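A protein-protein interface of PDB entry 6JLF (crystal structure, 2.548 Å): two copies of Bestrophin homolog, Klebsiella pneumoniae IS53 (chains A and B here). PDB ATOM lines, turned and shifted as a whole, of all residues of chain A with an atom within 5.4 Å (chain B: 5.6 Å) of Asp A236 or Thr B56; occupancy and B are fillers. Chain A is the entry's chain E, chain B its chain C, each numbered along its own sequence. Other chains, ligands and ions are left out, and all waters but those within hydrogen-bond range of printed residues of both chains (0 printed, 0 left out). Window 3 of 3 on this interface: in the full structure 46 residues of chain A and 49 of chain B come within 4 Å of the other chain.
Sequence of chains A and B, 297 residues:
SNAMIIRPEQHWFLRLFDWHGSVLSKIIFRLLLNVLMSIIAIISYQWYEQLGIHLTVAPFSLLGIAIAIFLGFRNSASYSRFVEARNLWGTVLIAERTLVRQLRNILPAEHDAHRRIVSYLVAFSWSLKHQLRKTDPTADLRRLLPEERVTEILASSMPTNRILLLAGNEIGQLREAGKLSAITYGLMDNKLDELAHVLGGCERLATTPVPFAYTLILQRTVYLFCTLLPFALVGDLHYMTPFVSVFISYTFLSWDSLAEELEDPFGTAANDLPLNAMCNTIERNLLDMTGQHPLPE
Of the printed residues of chain B, Val A57 touches Ala B58 (3.5 Å).
Of chain B, only His B54 (3.5 Å) and Thr B56 (3.0 Å) come within 4 Å of Asp A236.
Of the printed residues of chain B, His A238 touches His B54.
Of the printed residues of chain A, His B54 touches Asp A236, Leu A237 and His A238.
Of the printed residues of chain A, Leu B55 touches Leu A237.
Printed residues of chain A within 4 Å of Thr B56: Asp A236 (3.0 Å) and Leu A237 (3.6 Å).
Of the printed residues of chain A, Ala B58 touches Val A57 (3.5 Å).
The nearest printed residue of chain A that does not touch Thr B56 is Val A57 (5.4 Å).
Of the 9 printed residues of chain B, 4 touch a printed residue of chain A.
Hydrophobic or aromatic side chains of chain A that line the printed part of chain B: Val A57, Leu A237 and His A238.
Among the printed residues, 7 pairs touch across the chains.
Among the printed residues, no Asp or Glu carboxylate lies within 4 Å of a Lys or Arg side-chain nitrogen of the other chain.
Among the printed residues, pairs that only touch across the chains: Asp A236 with Thr B56 (3.0 Å), Leu A237 with His B54 (3.4 Å), Asp A236 with His B54 (3.5 Å), Val A57 with Ala B58 (3.5 Å), Leu A237 with Thr B56 (3.6 Å) and Leu A237 with Leu B55 (3.98 Å).
The backbone NH (N) of His A238 sits close to a ring nitrogen (ND1) of His B54 (3.5 Å).
The backbone carbonyl oxygen (O) of Gly A235 lies close to a ring nitrogen (NE2) of His A238, 3.2 Å away.
The backbone NH of Ala B58 is in hydrogen-bond range of the side-chain hydroxyl of Thr B56, at 3.4 Å.
Positions printed for both chains: 55, 57, 232 and 236.
Of the 7 pairs that touch across the chains among the printed residues, none has its exchanged pair printed and touching as well.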
ATOM      1  N   LEU A  55     -21.537 -23.760  10.674  1.00  0.00           N
ATOM      2  CA  LEU A  55     -21.262 -22.991   9.463  1.00  0.00           C
ATOM      3  C   LEU A  55     -22.585 -22.457   8.947  1.00  0.00           C
ATOM      4  O   LEU A  55     -23.479 -23.233   8.595  1.00  0.00           O
ATOM      5  CB  LEU A  55     -20.539 -23.830   8.407  1.00  0.00           C
ATOM      6  CG  LEU A  55     -19.044 -24.128   8.629  1.00  0.00           C
ATOM      7  CD1 LEU A  55     -18.502 -24.909   7.478  1.00  0.00           C
ATOM      8  CD2 LEU A  55     -18.182 -22.890   8.843  1.00  0.00           C
ATOM      9  N   VAL A  57     -24.716 -20.196   6.111  1.00  0.00           N
ATOM     10  CA  VAL A  57     -24.671 -19.746   4.727  1.00  0.00           C
ATOM     11  C   VAL A  57     -24.308 -18.261   4.644  1.00  0.00           C
ATOM     12  O   VAL A  57     -23.565 -17.857   3.746  1.00  0.00           O
ATOM     13  CB  VAL A  57     -26.019 -20.062   4.049  1.00  0.00           C
ATOM     14  CG1 VAL A  57     -26.140 -19.373   2.700  1.00  0.00           C
ATOM     15  CG2 VAL A  57     -26.201 -21.580   3.901  1.00  0.00           C
ATOM     16  N   ALA A 232     -20.915 -25.587   4.771  1.00  0.00           N
ATOM     17  CA  ALA A 232     -21.859 -24.561   5.194  1.00  0.00           C
ATOM     18  C   ALA A 232     -23.242 -24.754   4.593  1.00  0.00           C
ATOM     19  O   ALA A 232     -24.210 -24.163   5.079  1.00  0.00           O
ATOM     20  CB  ALA A 232     -21.335 -23.167   4.839  1.00  0.00           C
ATOM     21  N   LEU A 233     -23.362 -25.559   3.558  1.00  0.00           N
ATOM     22  CA  LEU A 233     -24.667 -25.823   2.979  1.00  0.00           C
ATOM     23  C   LEU A 233     -25.380 -26.996   3.644  1.00  0.00           C
ATOM     24  O   LEU A 233     -26.601 -27.146   3.467  1.00  0.00           O
ATOM     25  CB  LEU A 233     -24.531 -26.094   1.476  1.00  0.00           C
ATOM     26  CG  LEU A 233     -24.024 -24.944   0.623  1.00  0.00           C
ATOM     27  CD1 LEU A 233     -24.462 -25.182  -0.812  1.00  0.00           C
ATOM     28  CD2 LEU A 233     -24.541 -23.604   1.143  1.00  0.00           C
ATOM     29  N   VAL A 234     -24.640 -27.826   4.390  1.00  0.00           N
ATOM     30  CA  VAL A 234     -25.175 -29.096   4.868  1.00  0.00           C
ATOM     31  C   VAL A 234     -26.255 -28.867   5.921  1.00  0.00           C
ATOM     32  O   VAL A 234     -27.286 -29.549   5.927  1.00  0.00           O
ATOM     33  CB  VAL A 234     -24.034 -29.998   5.378  1.00  0.00           C
ATOM     34  CG1 VAL A 234     -23.465 -29.500   6.692  1.00  0.00           C
ATOM     35  CG2 VAL A 234     -24.500 -31.430   5.490  1.00  0.00           C
ATOM     36  N   GLY A 235     -26.060 -27.889   6.807  1.00  0.00           N
ATOM     37  CA  GLY A 235     -27.119 -27.543   7.737  1.00  0.00           C
ATOM     38  C   GLY A 235     -28.407 -27.162   7.027  1.00  0.00           C
ATOM     39  O   GLY A 235     -29.475 -27.698   7.323  1.00  0.00           O
ATOM     40  N   ASP A 236     -28.313 -26.254   6.056  1.00  0.00           N
ATOM     41  CA  ASP A 236     -29.503 -25.780   5.353  1.00  0.00           C
ATOM     42  C   ASP A 236     -30.119 -26.862   4.477  1.00  0.00           C
ATOM     43  O   ASP A 236     -31.344 -26.974   4.395  1.00  0.00           O
ATOM     44  CB  ASP A 236     -29.146 -24.579   4.476  1.00  0.00           C
ATOM     45  CG  ASP A 236     -29.086 -23.269   5.241  1.00  0.00           C
ATOM     46  OD1 ASP A 236     -28.254 -23.142   6.178  1.00  0.00           O
ATOM     47  OD2 ASP A 236     -29.860 -22.353   4.869  1.00  0.00           O
ATOM     48  N   LEU A 237     -29.291 -27.640   3.802  1.00  0.00           N
ATOM     49  CA  LEU A 237     -29.714 -28.631   2.821  1.00  0.00           C
ATOM     50  C   LEU A 237     -29.211 -29.946   3.391  1.00  0.00           C
ATOM     51  O   LEU A 237     -28.011 -30.110   3.584  1.00  0.00           O
ATOM     52  CB  LEU A 237     -29.086 -28.344   1.452  1.00  0.00           C
ATOM     53  CG  LEU A 237     -28.763 -26.912   0.976  1.00  0.00           C
ATOM     54  CD1 LEU A 237     -28.044 -26.958  -0.339  1.00  0.00           C
ATOM     55  CD2 LEU A 237     -30.009 -26.038   0.821  1.00  0.00           C
ATOM     56  N   HIS A 238     -30.094 -30.850   3.777  1.00  0.00           N
ATOM     57  CA  HIS A 238     -29.533 -31.990   4.489  1.00  0.00           C
ATOM     58  C   HIS A 238     -28.886 -32.941   3.478  1.00  0.00           C
ATOM     59  O   HIS A 238     -27.654 -33.000   3.376  1.00  0.00           O
ATOM     60  CB  HIS A 238     -30.614 -32.621   5.404  1.00  0.00           C
ATOM     61  CG  HIS A 238     -30.950 -31.788   6.635  1.00  0.00           C
ATOM     62  ND1 HIS A 238     -31.458 -32.329   7.803  1.00  0.00           N
ATOM     63  CD2 HIS A 238     -30.848 -30.449   6.865  1.00  0.00           C
ATOM     64  CE1 HIS A 238     -31.635 -31.365   8.697  1.00  0.00           C
ATOM     65  NE2 HIS A 238     -31.279 -30.217   8.153  1.00  0.00           N
ATOM     66  N   HIS B  54     -33.704 -30.576   1.441  1.00  0.00           N
ATOM     67  CA  HIS B  54     -34.239 -29.245   1.700  1.00  0.00           C
ATOM     68  C   HIS B  54     -33.569 -28.231   0.782  1.00  0.00           C
ATOM     69  O   HIS B  54     -32.411 -28.403   0.391  1.00  0.00           O
ATOM     70  CB  HIS B  54     -34.035 -28.833   3.170  1.00  0.00           C
ATOM     71  CG  HIS B  54     -34.218 -29.955   4.154  1.00  0.00           C
ATOM     72  ND1 HIS B  54     -33.256 -30.306   5.072  1.00  0.00           N
ATOM     73  CD2 HIS B  54     -35.257 -30.799   4.362  1.00  0.00           C
ATOM     74  CE1 HIS B  54     -33.688 -31.324   5.794  1.00  0.00           C
ATOM     75  NE2 HIS B  54     -34.896 -31.648   5.379  1.00  0.00           N
ATOM     76  N   LEU B  55     -34.309 -27.184   0.420  1.00  0.00           N
ATOM     77  CA  LEU B  55     -33.790 -26.113  -0.432  1.00  0.00           C
ATOM     78  C   LEU B  55     -34.183 -24.777   0.179  1.00  0.00           C
ATOM     79  O   LEU B  55     -35.343 -24.368   0.105  1.00  0.00           O
ATOM     80  CB  LEU B  55     -34.295 -26.241  -1.863  1.00  0.00           C
ATOM     81  CG  LEU B  55     -33.412 -27.180  -2.692  1.00  0.00           C
ATOM     82  CD1 LEU B  55     -34.136 -27.589  -3.960  1.00  0.00           C
ATOM     83  CD2 LEU B  55     -32.039 -26.557  -3.009  1.00  0.00           C
ATOM     84  N   THR B  56     -33.231 -24.127   0.826  1.00  0.00           N
ATOM     85  CA  THR B  56     -33.477 -22.796   1.333  1.00  0.00           C
ATOM     86  C   THR B  56     -33.259 -21.773   0.226  1.00  0.00           C
ATOM     87  O   THR B  56     -32.904 -22.097  -0.909  1.00  0.00           O
ATOM     88  CB  THR B  56     -32.586 -22.521   2.545  1.00  0.00           C
ATOM     89  OG1 THR B  56     -32.580 -21.116   2.859  1.00  0.00           O
ATOM     90  CG2 THR B  56     -31.210 -22.985   2.279  1.00  0.00           C
ATOM     91  N   VAL B  57     -33.510 -20.516   0.564  1.00  0.00           N
ATOM     92  CA  VAL B  57     -33.356 -19.454  -0.408  1.00  0.00           C
ATOM     93  C   VAL B  57     -31.946 -18.874  -0.402  1.00  0.00           C
ATOM     94  O   VAL B  57     -31.426 -18.538  -1.474  1.00  0.00           O
ATOM     95  CB  VAL B  57     -34.422 -18.376  -0.137  1.00  0.00           C
ATOM     96  CG1 VAL B  57     -34.017 -17.046  -0.677  1.00  0.00           C
ATOM     97  CG2 VAL B  57     -35.745 -18.798  -0.739  1.00  0.00           C
ATOM     98  N   ALA B  58     -31.293 -18.806   0.758  1.00  0.00           N
ATOM     99  CA  ALA B  58     -29.966 -18.187   0.841  1.00  0.00           C
ATOM    100  C   ALA B  58     -28.917 -18.767  -0.120  1.00  0.00           C
ATOM    101  O   ALA B  58     -28.159 -17.968  -0.717  1.00  0.00           O
ATOM    102  CB  ALA B  58     -29.449 -18.265   2.285  1.00  0.00           C
ATOM    103  N   PRO B  59     -28.775 -20.089  -0.303  1.00  0.00           N
ATOM    104  CA  PRO B  59     -27.790 -20.568  -1.290  1.00  0.00           C
ATOM    105  C   PRO B  59     -28.125 -20.134  -2.705  1.00  0.00           C
ATOM    106  O   PRO B  59     -27.241 -19.733  -3.467  1.00  0.00           O
ATOM    107  CB  PRO B  59     -27.851 -22.100  -1.155  1.00  0.00           C
ATOM    108  CG  PRO B  59     -28.585 -22.364   0.082  1.00  0.00           C
ATOM    109  CD  PRO B  59     -29.521 -21.213   0.280  1.00  0.00           C
ATOM    110  N   PHE B  60     -29.390 -20.215  -3.084  1.00  0.00           N
ATOM    111  CA  PHE B  60     -29.785 -19.744  -4.396  1.00  0.00           C
ATOM    112  C   PHE B  60     -29.768 -18.229  -4.512  1.00  0.00           C
ATOM    113  O   PHE B  60     -29.829 -17.714  -5.629  1.00  0.00           O
ATOM    114  CB  PHE B  60     -31.161 -20.291  -4.742  1.00  0.00           C
ATOM    115  CG  PHE B  60     -31.116 -21.684  -5.254  1.00  0.00           C
ATOM    116  CD1 PHE B  60     -30.675 -22.715  -4.438  1.00  0.00           C
ATOM    117  CD2 PHE B  60     -31.475 -21.970  -6.560  1.00  0.00           C
ATOM    118  CE1 PHE B  60     -30.609 -24.021  -4.908  1.00  0.00           C
ATOM    119  CE2 PHE B  60     -31.415 -23.275  -7.042  1.00  0.00           C
ATOM    120  CZ  PHE B  60     -30.979 -24.303  -6.212  1.00  0.00           C
ATOM    121  N   ALA B 232     -36.352 -24.068  -4.657  1.00  0.00           N
ATOM    122  CA  ALA B 232     -35.776 -23.319  -3.553  1.00  0.00           C
ATOM    123  C   ALA B 232     -36.665 -22.180  -3.086  1.00  0.00           C
ATOM    124  O   ALA B 232     -36.351 -21.542  -2.085  1.00  0.00           O
ATOM    125  CB  ALA B 232     -34.408 -22.758  -3.942  1.00  0.00           C
ATOM    126  N   ASP B 236     -40.231 -20.730   1.370  1.00  0.00           N
ATOM    127  CA  ASP B 236     -40.433 -19.366   1.851  1.00  0.00           C
ATOM    128  C   ASP B 236     -41.785 -18.820   1.404  1.00  0.00           C
ATOM    129  O   ASP B 236     -42.444 -18.098   2.156  1.00  0.00           O
ATOM    130  CB  ASP B 236     -39.314 -18.442   1.347  1.00  0.00           C
ATOM    131  CG  ASP B 236     -38.106 -18.393   2.277  1.00  0.00           C
ATOM    132  OD1 ASP B 236     -37.642 -19.474   2.725  1.00  0.00           O
ATOM    133  OD2 ASP B 236     -37.606 -17.259   2.527  1.00  0.00           O
